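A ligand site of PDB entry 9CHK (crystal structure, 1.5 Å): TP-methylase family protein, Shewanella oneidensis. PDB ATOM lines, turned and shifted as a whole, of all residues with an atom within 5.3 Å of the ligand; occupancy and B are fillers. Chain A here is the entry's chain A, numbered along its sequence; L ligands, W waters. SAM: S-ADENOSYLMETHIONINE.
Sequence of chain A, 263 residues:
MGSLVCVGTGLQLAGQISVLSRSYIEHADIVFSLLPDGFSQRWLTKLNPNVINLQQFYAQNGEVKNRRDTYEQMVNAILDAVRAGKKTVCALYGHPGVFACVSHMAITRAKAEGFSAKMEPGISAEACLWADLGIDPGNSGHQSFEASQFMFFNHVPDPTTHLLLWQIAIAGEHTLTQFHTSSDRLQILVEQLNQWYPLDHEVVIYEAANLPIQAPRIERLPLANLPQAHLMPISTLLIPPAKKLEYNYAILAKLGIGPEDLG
The backbone carbonyl oxygen (O) of Phe 99 sits close to a sulfur (SD) of the ligand (2.9 Å).
A nitrogen (N3) of the ligand sits close to the backbone carbonyl oxygen (O) of Ile 234, at 2.9 Å.
Leu 11 touches the ligand (CD1 to N6, 3.8 Å).
OH of Tyr 93 touches CG of the ligand (3.1 Å).
Gly 94 touches the ligand.
Ser 124 touches the ligand.
Trp 166 touches the ligand (CA to O2', 3.4 Å).
O of Tyr 206 touches C2 of the ligand, 3.6 Å away.
Glu 207 touches the ligand (CA to N1, 3.4 Å).
Of the 26 residues printed, 17 come within 4 Å of the ligand.
Along chain A the residues within 4 Å of the ligand span positions 11 to 236.
The nearest printed residue that does not touch the ligand is Ala 100 (4.2 Å).
Water W1 lies within hydrogen-bond range of N7 of the ligand (2.9 Å) and OD1 of Asn 210 (3.0 Å).
Water W2 lies within hydrogen-bond range of the backbone carbonyl oxygen (O) of Ser 235 (2.8 Å), the backbone carbonyl oxygen (O) of Pro 233 (3.1 Å), the backbone NH (N) of Ile 168 (3.3 Å) and an oxygen (O3') of the ligand (3.5 Å).
N of Ala 208 is in hydrogen-bond range of N1 of the ligand, 2.8 Å away.
The backbone carbonyl oxygen (O) of His 95 sits at hydrogen-bond distance from a nitrogen (N) of the ligand, at 2.9 Å.
An oxygen (O2') of the ligand sits at hydrogen-bond distance from the backbone carbonyl oxygen (O) of Ser 235, 3.3 Å away.
An oxygen (O3') of the ligand sits at hydrogen-bond distance from the backbone carbonyl oxygen (O) of Pro 233.
O of Val 98 lies within hydrogen-bond range of N of the ligand, at 2.8 Å.
An oxygen (O2') of the ligand is in hydrogen-bond range of the side-chain hydroxyl of Thr 236 (2.7 Å).
A nitrogen (N6) of the ligand lies within hydrogen-bond range of the backbone carbonyl oxygen (O) of Ala 208.
An oxygen (O2') of the ligand is in hydrogen-bond range of the backbone NH of Gln 167 (3.0 Å).
The backbone NH (N) of Ala 125 sits at hydrogen-bond distance from an oxygen (O) of the ligand (2.9 Å).
An oxygen (OXT) of the ligand lies within hydrogen-bond range of the backbone NH (N) of His 95 (2.8 Å).
The side-chain hydroxyl of Ser 124 sits close to the backbone NH of Glu 126.
The backbone carbonyl oxygen of Thr 236 lies within hydrogen-bond range of the backbone NH of Tyr 206 (2.9 Å).
OD1 of Asn 210 sits close to O of Leu 11.
The side-chain hydroxyl of Ser 235 lies within hydrogen-bond range of the side-chain carboxylate of Glu 207, 2.6 Å away.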
ATOM      1  N   LEU A  11     -17.595  14.570 -28.812  1.00  0.00           N
ATOM      2  CA  LEU A  11     -18.796  15.341 -28.531  1.00  0.00           C
ATOM      3  C   LEU A  11     -19.851  15.121 -29.614  1.00  0.00           C
ATOM      4  O   LEU A  11     -21.038  15.085 -29.316  1.00  0.00           O
ATOM      5  CB  LEU A  11     -18.439  16.817 -28.364  1.00  0.00           C
ATOM      6  CG  LEU A  11     -17.625  17.156 -27.121  1.00  0.00           C
ATOM      7  CD1 LEU A  11     -17.574  18.656 -26.906  1.00  0.00           C
ATOM      8  CD2 LEU A  11     -18.176  16.454 -25.884  1.00  0.00           C
ATOM      9  N   TYR A  71     -20.770  10.095  -8.145  1.00  0.00           N
ATOM     10  CA  TYR A  71     -19.548   9.656  -8.795  1.00  0.00           C
ATOM     11  C   TYR A  71     -19.055   8.366  -8.149  1.00  0.00           C
ATOM     12  O   TYR A  71     -18.615   7.452  -8.841  1.00  0.00           O
ATOM     13  CB  TYR A  71     -18.476  10.757  -8.740  1.00  0.00           C
ATOM     14  CG  TYR A  71     -18.821  11.999  -9.539  1.00  0.00           C
ATOM     15  CD1 TYR A  71     -19.667  11.938 -10.640  1.00  0.00           C
ATOM     16  CD2 TYR A  71     -18.300  13.242  -9.187  1.00  0.00           C
ATOM     17  CE1 TYR A  71     -19.984  13.071 -11.368  1.00  0.00           C
ATOM     18  CE2 TYR A  71     -18.605  14.382  -9.913  1.00  0.00           C
ATOM     19  CZ  TYR A  71     -19.461  14.292 -11.009  1.00  0.00           C
ATOM     20  OH  TYR A  71     -19.769  15.419 -11.717  1.00  0.00           O
ATOM     21  N   TYR A  93     -18.526  10.710 -22.720  1.00  0.00           N
ATOM     22  CA  TYR A  93     -18.479  11.680 -23.789  1.00  0.00           C
ATOM     23  C   TYR A  93     -17.194  12.484 -23.647  1.00  0.00           C
ATOM     24  O   TYR A  93     -16.645  12.651 -22.553  1.00  0.00           O
ATOM     25  CB  TYR A  93     -19.737  12.561 -23.831  1.00  0.00           C
ATOM     26  CG  TYR A  93     -19.824  13.618 -22.749  1.00  0.00           C
ATOM     27  CD1 TYR A  93     -20.430  13.348 -21.531  1.00  0.00           C
ATOM     28  CD2 TYR A  93     -19.330  14.892 -22.956  1.00  0.00           C
ATOM     29  CE1 TYR A  93     -20.534  14.314 -20.546  1.00  0.00           C
ATOM     30  CE2 TYR A  93     -19.412  15.865 -21.974  1.00  0.00           C
ATOM     31  CZ  TYR A  93     -20.025  15.580 -20.768  1.00  0.00           C
ATOM     32  OH  TYR A  93     -20.113  16.525 -19.796  1.00  0.00           O
ATOM     33  N   GLY A  94     -16.702  12.966 -24.799  1.00  0.00           N
ATOM     34  CA  GLY A  94     -15.497  13.774 -24.854  1.00  0.00           C
ATOM     35  C   GLY A  94     -14.249  12.908 -24.691  1.00  0.00           C
ATOM     36  O   GLY A  94     -14.131  11.850 -25.304  1.00  0.00           O
ATOM     37  N   HIS A  95     -13.342  13.406 -23.858  1.00  0.00           N
ATOM     38  CA  HIS A  95     -12.170  12.686 -23.401  1.00  0.00           C
ATOM     39  C   HIS A  95     -12.468  12.187 -21.995  1.00  0.00           C
ATOM     40  O   HIS A  95     -12.898  12.968 -21.146  1.00  0.00           O
ATOM     41  CB  HIS A  95     -10.984  13.652 -23.440  1.00  0.00           C
ATOM     42  CG  HIS A  95      -9.673  13.106 -22.986  1.00  0.00           C
ATOM     43  ND1 HIS A  95      -9.474  12.339 -21.862  1.00  0.00           N
ATOM     44  CD2 HIS A  95      -8.460  13.290 -23.530  1.00  0.00           C
ATOM     45  CE1 HIS A  95      -8.184  12.072 -21.740  1.00  0.00           C
ATOM     46  NE2 HIS A  95      -7.542  12.644 -22.747  1.00  0.00           N
ATOM     47  N   PRO A  96     -12.294  10.883 -21.700  1.00  0.00           N
ATOM     48  CA  PRO A  96     -12.780  10.330 -20.431  1.00  0.00           C
ATOM     49  C   PRO A  96     -12.028  10.826 -19.197  1.00  0.00           C
ATOM     50  O   PRO A  96     -12.447  10.553 -18.074  1.00  0.00           O
ATOM     51  CB  PRO A  96     -12.595   8.819 -20.638  1.00  0.00           C
ATOM     52  CG  PRO A  96     -11.412   8.726 -21.576  1.00  0.00           C
ATOM     53  CD  PRO A  96     -11.613   9.885 -22.531  1.00  0.00           C
ATOM     54  N   VAL A  98     -10.800  14.243 -18.970  1.00  0.00           N
ATOM     55  CA  VAL A  98     -10.761  15.702 -18.966  1.00  0.00           C
ATOM     56  C   VAL A  98     -11.997  16.251 -18.260  1.00  0.00           C
ATOM     57  O   VAL A  98     -13.116  16.076 -18.728  1.00  0.00           O
ATOM     58  CB  VAL A  98     -10.622  16.231 -20.408  1.00  0.00           C
ATOM     59  CG1 VAL A  98     -10.857  17.733 -20.497  1.00  0.00           C
ATOM     60  CG2 VAL A  98      -9.266  15.872 -20.992  1.00  0.00           C
ATOM     61  N   PHE A  99     -11.766  16.922 -17.119  1.00  0.00           N
ATOM     62  CA  PHE A  99     -12.853  17.405 -16.277  1.00  0.00           C
ATOM     63  C   PHE A  99     -13.836  16.263 -16.043  1.00  0.00           C
ATOM     64  O   PHE A  99     -15.050  16.428 -16.179  1.00  0.00           O
ATOM     65  CB  PHE A  99     -13.472  18.664 -16.885  1.00  0.00           C
ATOM     66  CG  PHE A  99     -12.589  19.881 -16.724  1.00  0.00           C
ATOM     67  CD1 PHE A  99     -11.557  20.141 -17.617  1.00  0.00           C
ATOM     68  CD2 PHE A  99     -12.738  20.742 -15.635  1.00  0.00           C
ATOM     69  CE1 PHE A  99     -10.721  21.238 -17.452  1.00  0.00           C
ATOM     70  CE2 PHE A  99     -11.917  21.839 -15.478  1.00  0.00           C
ATOM     71  CZ  PHE A  99     -10.900  22.084 -16.379  1.00  0.00           C
ATOM     72  N   ALA A 100     -13.282  15.105 -15.659  1.00  0.00           N
ATOM     73  CA  ALA A 100     -14.041  13.887 -15.432  1.00  0.00           C
ATOM     74  C   ALA A 100     -13.273  13.030 -14.428  1.00  0.00           C
ATOM     75  O   ALA A 100     -12.155  12.608 -14.710  1.00  0.00           O
ATOM     76  CB  ALA A 100     -14.233  13.148 -16.744  1.00  0.00           C
ATOM     77  N   ILE A 123     -11.577  13.104 -27.917  1.00  0.00           N
ATOM     78  CA  ILE A 123     -11.679  14.493 -28.304  1.00  0.00           C
ATOM     79  C   ILE A 123     -12.572  15.228 -27.307  1.00  0.00           C
ATOM     80  O   ILE A 123     -13.755  14.927 -27.185  1.00  0.00           O
ATOM     81  CB  ILE A 123     -12.194  14.588 -29.756  1.00  0.00           C
ATOM     82  CG1 ILE A 123     -11.151  14.028 -30.731  1.00  0.00           C
ATOM     83  CG2 ILE A 123     -12.610  16.014 -30.108  1.00  0.00           C
ATOM     84  CD1 ILE A 123     -11.680  13.744 -32.126  1.00  0.00           C
ATOM     85  N   SER A 124     -11.977  16.207 -26.601  1.00  0.00           N
ATOM     86  CA  SER A 124     -12.644  16.929 -25.521  1.00  0.00           C
ATOM     87  C   SER A 124     -13.345  18.181 -26.044  1.00  0.00           C
ATOM     88  O   SER A 124     -13.193  18.556 -27.204  1.00  0.00           O
ATOM     89  CB  SER A 124     -11.646  17.311 -24.459  1.00  0.00           C
ATOM     90  OG  SER A 124     -10.817  18.365 -24.921  1.00  0.00           O
ATOM     91  N   ALA A 125     -14.106  18.829 -25.158  1.00  0.00           N
ATOM     92  CA  ALA A 125     -14.794  20.064 -25.484  1.00  0.00           C
ATOM     93  C   ALA A 125     -13.802  21.144 -25.930  1.00  0.00           C
ATOM     94  O   ALA A 125     -14.119  21.942 -26.813  1.00  0.00           O
ATOM     95  CB  ALA A 125     -15.614  20.540 -24.304  1.00  0.00           C
ATOM     96  N   GLU A 126     -12.610  21.184 -25.316  1.00  0.00           N
ATOM     97  CA  GLU A 126     -11.653  22.222 -25.642  1.00  0.00           C
ATOM     98  C   GLU A 126     -11.033  21.931 -27.011  1.00  0.00           C
ATOM     99  O   GLU A 126     -10.799  22.844 -27.790  1.00  0.00           O
ATOM    100  CB  GLU A 126     -10.652  22.480 -24.513  1.00  0.00           C
ATOM    101  CG  GLU A 126      -9.534  21.454 -24.352  1.00  0.00           C
ATOM    102  CD  GLU A 126      -8.524  21.857 -23.288  1.00  0.00           C
ATOM    103  OE1 GLU A 126      -8.817  22.794 -22.518  1.00  0.00           O
ATOM    104  OE2 GLU A 126      -7.433  21.256 -23.253  1.00  0.00           O
ATOM    105  N   LEU A 165     -13.074  28.719 -18.534  1.00  0.00           N
ATOM    106  CA  LEU A 165     -13.736  28.366 -17.286  1.00  0.00           C
ATOM    107  C   LEU A 165     -14.785  27.301 -17.580  1.00  0.00           C
ATOM    108  O   LEU A 165     -15.771  27.564 -18.257  1.00  0.00           O
ATOM    109  CB  LEU A 165     -14.349  29.587 -16.615  1.00  0.00           C
ATOM    110  CG  LEU A 165     -13.359  30.645 -16.113  1.00  0.00           C
ATOM    111  CD1 LEU A 165     -14.122  31.744 -15.397  1.00  0.00           C
ATOM    112  CD2 LEU A 165     -12.303  30.039 -15.202  1.00  0.00           C
ATOM    113  N   TRP A 166     -14.522  26.083 -17.104  1.00  0.00           N
ATOM    114  CA  TRP A 166     -15.388  24.940 -17.330  1.00  0.00           C
ATOM    115  C   TRP A 166     -16.481  24.898 -16.256  1.00  0.00           C
ATOM    116  O   TRP A 166     -16.286  25.412 -15.154  1.00  0.00           O
ATOM    117  CB  TRP A 166     -14.573  23.643 -17.296  1.00  0.00           C
ATOM    118  CG  TRP A 166     -13.515  23.510 -18.353  1.00  0.00           C
ATOM    119  CD1 TRP A 166     -12.409  24.292 -18.525  1.00  0.00           C
ATOM    120  CD2 TRP A 166     -13.419  22.472 -19.347  1.00  0.00           C
ATOM    121  NE1 TRP A 166     -11.662  23.839 -19.578  1.00  0.00           N
ATOM    122  CE2 TRP A 166     -12.240  22.709 -20.089  1.00  0.00           C
ATOM    123  CE3 TRP A 166     -14.208  21.364 -19.674  1.00  0.00           C
ATOM    124  CZ2 TRP A 166     -11.853  21.881 -21.142  1.00  0.00           C
ATOM    125  CZ3 TRP A 166     -13.824  20.551 -20.712  1.00  0.00           C
ATOM    126  CH2 TRP A 166     -12.651  20.790 -21.419  1.00  0.00           C
ATOM    127  N   GLN A 167     -17.605  24.258 -16.567  1.00  0.00           N
ATOM    128  CA  GLN A 167     -18.678  24.081 -15.604  1.00  0.00           C
ATOM    129  C   GLN A 167     -19.154  25.452 -15.106  1.00  0.00           C
ATOM    130  O   GLN A 167     -19.473  25.612 -13.934  1.00  0.00           O
ATOM    131  CB  GLN A 167     -18.220  23.138 -14.498  1.00  0.00           C
ATOM    132  CG  GLN A 167     -17.744  21.792 -15.045  1.00  0.00           C
ATOM    133  CD  GLN A 167     -17.672  20.682 -14.016  1.00  0.00           C
ATOM    134  OE1 GLN A 167     -17.533  20.892 -12.811  1.00  0.00           O
ATOM    135  NE2 GLN A 167     -17.734  19.450 -14.521  1.00  0.00           N
ATOM    136  N   ILE A 168     -19.271  26.399 -16.027  1.00  0.00           N
ATOM    137  CA  ILE A 168     -19.647  27.766 -15.693  1.00  0.00           C
ATOM    138  C   ILE A 168     -21.079  27.798 -15.167  1.00  0.00           C
ATOM    139  O   ILE A 168     -21.410  28.646 -14.351  1.00  0.00           O
ATOM    140  CB  ILE A 168     -19.423  28.689 -16.897  1.00  0.00           C
ATOM    141  CG1 ILE A 168     -19.609  30.166 -16.547  1.00  0.00           C
ATOM    142  CG2 ILE A 168     -20.302  28.291 -18.084  1.00  0.00           C
ATOM    143  CD1 ILE A 168     -18.599  30.700 -15.545  1.00  0.00           C
ATOM    144  N   TYR A 206     -19.424  29.119 -25.143  1.00  0.00           N
ATOM    145  CA  TYR A 206     -19.218  28.133 -26.190  1.00  0.00           C
ATOM    146  C   TYR A 206     -19.910  26.822 -25.834  1.00  0.00           C
ATOM    147  O   TYR A 206     -19.763  26.310 -24.729  1.00  0.00           O
ATOM    148  CB  TYR A 206     -17.732  27.890 -26.434  1.00  0.00           C
ATOM    149  CG  TYR A 206     -17.452  26.731 -27.375  1.00  0.00           C
ATOM    150  CD1 TYR A 206     -17.705  26.833 -28.739  1.00  0.00           C
ATOM    151  CD2 TYR A 206     -16.926  25.529 -26.905  1.00  0.00           C
ATOM    152  CE1 TYR A 206     -17.474  25.785 -29.607  1.00  0.00           C
ATOM    153  CE2 TYR A 206     -16.681  24.467 -27.764  1.00  0.00           C
ATOM    154  CZ  TYR A 206     -16.942  24.598 -29.125  1.00  0.00           C
ATOM    155  OH  TYR A 206     -16.697  23.545 -29.961  1.00  0.00           O
ATOM    156  N   GLU A 207     -20.633  26.283 -26.814  1.00  0.00           N
ATOM    157  CA  GLU A 207     -21.155  24.931 -26.730  1.00  0.00           C
ATOM    158  C   GLU A 207     -20.864  24.210 -28.049  1.00  0.00           C
ATOM    159  O   GLU A 207     -21.397  24.578 -29.091  1.00  0.00           O
ATOM    160  CB  GLU A 207     -22.659  24.930 -26.426  1.00  0.00           C
ATOM    161  CG  GLU A 207     -22.977  25.527 -25.058  1.00  0.00           C
ATOM    162  CD  GLU A 207     -24.444  25.826 -24.825  1.00  0.00           C
ATOM    163  OE1 GLU A 207     -25.290  25.371 -25.626  1.00  0.00           O
ATOM    164  OE2 GLU A 207     -24.739  26.541 -23.847  1.00  0.00           O
ATOM    165  N   ALA A 208     -19.992  23.205 -27.969  1.00  0.00           N
ATOM    166  CA  ALA A 208     -19.772  22.299 -29.089  1.00  0.00           C
ATOM    167  C   ALA A 208     -21.067  21.570 -29.402  1.00  0.00           C
ATOM    168  O   ALA A 208     -21.809  21.186 -28.490  1.00  0.00           O
ATOM    169  CB  ALA A 208     -18.657  21.333 -28.750  1.00  0.00           C
ATOM    170  N   ALA A 209     -21.326  21.379 -30.701  1.00  0.00           N
ATOM    171  CA  ALA A 209     -22.473  20.617 -31.168  1.00  0.00           C
ATOM    172  C   ALA A 209     -22.311  19.138 -30.834  1.00  0.00           C
ATOM    173  O   ALA A 209     -21.212  18.603 -30.884  1.00  0.00           O
ATOM    174  CB  ALA A 209     -22.648  20.816 -32.658  1.00  0.00           C
ATOM    175  N   ASN A 210     -23.442  18.484 -30.540  1.00  0.00           N
ATOM    176  CA  ASN A 210     -23.457  17.056 -30.260  1.00  0.00           C
ATOM    177  C   ASN A 210     -24.070  16.284 -31.428  1.00  0.00           C
ATOM    178  O   ASN A 210     -23.958  15.061 -31.467  1.00  0.00           O
ATOM    179  CB  ASN A 210     -24.224  16.736 -28.980  1.00  0.00           C
ATOM    180  CG  ASN A 210     -23.551  17.283 -27.751  1.00  0.00           C
ATOM    181  OD1 ASN A 210     -22.423  16.890 -27.422  1.00  0.00           O
ATOM    182  ND2 ASN A 210     -24.221  18.181 -27.053  1.00  0.00           N
ATOM    183  N   PRO A 233     -25.628  23.158 -18.665  1.00  0.00           N
ATOM    184  CA  PRO A 233     -24.585  22.268 -18.132  1.00  0.00           C
ATOM    185  C   PRO A 233     -23.383  22.111 -19.069  1.00  0.00           C
ATOM    186  O   PRO A 233     -22.264  21.902 -18.612  1.00  0.00           O
ATOM    187  CB  PRO A 233     -25.357  20.956 -17.950  1.00  0.00           C
ATOM    188  CG  PRO A 233     -26.752  21.424 -17.579  1.00  0.00           C
ATOM    189  CD  PRO A 233     -26.988  22.630 -18.473  1.00  0.00           C
ATOM    190  N   ILE A 234     -23.624  22.209 -20.382  1.00  0.00           N
ATOM    191  CA  ILE A 234     -22.575  21.939 -21.351  1.00  0.00           C
ATOM    192  C   ILE A 234     -21.817  23.212 -21.728  1.00  0.00           C
ATOM    193  O   ILE A 234     -20.882  23.146 -22.536  1.00  0.00           O
ATOM    194  CB  ILE A 234     -23.142  21.260 -22.623  1.00  0.00           C
ATOM    195  CG1 ILE A 234     -24.268  22.089 -23.255  1.00  0.00           C
ATOM    196  CG2 ILE A 234     -23.586  19.827 -22.314  1.00  0.00           C
ATOM    197  CD1 ILE A 234     -24.678  21.605 -24.633  1.00  0.00           C
ATOM    198  N   SER A 235     -22.183  24.358 -21.160  1.00  0.00           N
ATOM    199  CA  SER A 235     -21.538  25.621 -21.516  1.00  0.00           C
ATOM    200  C   SER A 235     -20.116  25.674 -20.956  1.00  0.00           C
ATOM    201  O   SER A 235     -19.882  25.312 -19.797  1.00  0.00           O
ATOM    202  CB  SER A 235     -22.325  26.800 -21.003  1.00  0.00           C
ATOM    203  OG  SER A 235     -23.674  26.794 -21.459  1.00  0.00           O
ATOM    204  N   THR A 236     -19.188  26.159 -21.788  1.00  0.00           N
ATOM    205  CA  THR A 236     -17.859  26.547 -21.341  1.00  0.00           C
ATOM    206  C   THR A 236     -17.673  28.028 -21.641  1.00  0.00           C
ATOM    207  O   THR A 236     -18.065  28.512 -22.701  1.00  0.00           O
ATOM    208  CB  THR A 236     -16.789  25.698 -22.041  1.00  0.00           C
ATOM    209  OG1 THR A 236     -16.903  24.345 -21.601  1.00  0.00           O
ATOM    210  CG2 THR A 236     -15.391  26.190 -21.742  1.00  0.00           C
HETATM  211  N   SAM L   1     -14.949  14.922 -20.441  1.00  0.00           N
HETATM  212  CA  SAM L   1     -15.655  16.085 -21.035  1.00  0.00           C
HETATM  213  C   SAM L   1     -14.815  16.622 -22.204  1.00  0.00           C
HETATM  214  O   SAM L   1     -15.125  17.734 -22.676  1.00  0.00           O
HETATM  215  OXT SAM L   1     -13.886  15.900 -22.602  1.00  0.00           O
HETATM  216  CB  SAM L   1     -15.892  17.185 -19.995  1.00  0.00           C
HETATM  217  CG  SAM L   1     -17.082  16.917 -19.059  1.00  0.00           C
HETATM  218  SD  SAM L   1     -17.135  17.955 -17.570  1.00  0.00           S
HETATM  219  CE  SAM L   1     -17.945  16.849 -16.419  1.00  0.00           C
HETATM  220  C5' SAM L   1     -18.520  19.011 -18.046  1.00  0.00           C
HETATM  221  C4' SAM L   1     -18.038  20.328 -18.617  1.00  0.00           C
HETATM  222  O4' SAM L   1     -17.360  20.092 -19.866  1.00  0.00           O
HETATM  223  C3' SAM L   1     -19.132  21.329 -18.960  1.00  0.00           C
HETATM  224  O3' SAM L   1     -19.585  22.016 -17.798  1.00  0.00           O
HETATM  225  C2' SAM L   1     -18.360  22.227 -19.934  1.00  0.00           C
HETATM  226  O2' SAM L   1     -17.448  23.082 -19.293  1.00  0.00           O
HETATM  227  C1' SAM L   1     -17.620  21.165 -20.751  1.00  0.00           C
HETATM  228  N9  SAM L   1     -18.417  20.676 -21.870  1.00  0.00           N
HETATM  229  C8  SAM L   1     -19.152  19.518 -21.931  1.00  0.00           C
HETATM  230  N7  SAM L   1     -19.821  19.396 -23.050  1.00  0.00           N
HETATM  231  C5  SAM L   1     -19.537  20.560 -23.747  1.00  0.00           C
HETATM  232  C6  SAM L   1     -19.949  21.033 -25.016  1.00  0.00           C
HETATM  233  N6  SAM L   1     -20.779  20.373 -25.807  1.00  0.00           N
HETATM  234  N1  SAM L   1     -19.477  22.233 -25.405  1.00  0.00           N
HETATM  235  C2  SAM L   1     -18.656  22.902 -24.586  1.00  0.00           C
HETATM  236  N3  SAM L   1     -18.196  22.552 -23.393  1.00  0.00           N
HETATM  237  C4  SAM L   1     -18.678  21.357 -23.024  1.00  0.00           C
HETATM  238  O   HOH W   1     -21.602  17.668 -24.618  1.00  0.00           O
HETATM  239  O   HOH W   2     -21.619  24.818 -17.712  1.00  0.00           O
HETATM  240  O   HOH W   3     -21.022  15.643 -17.384  1.00  0.00           O
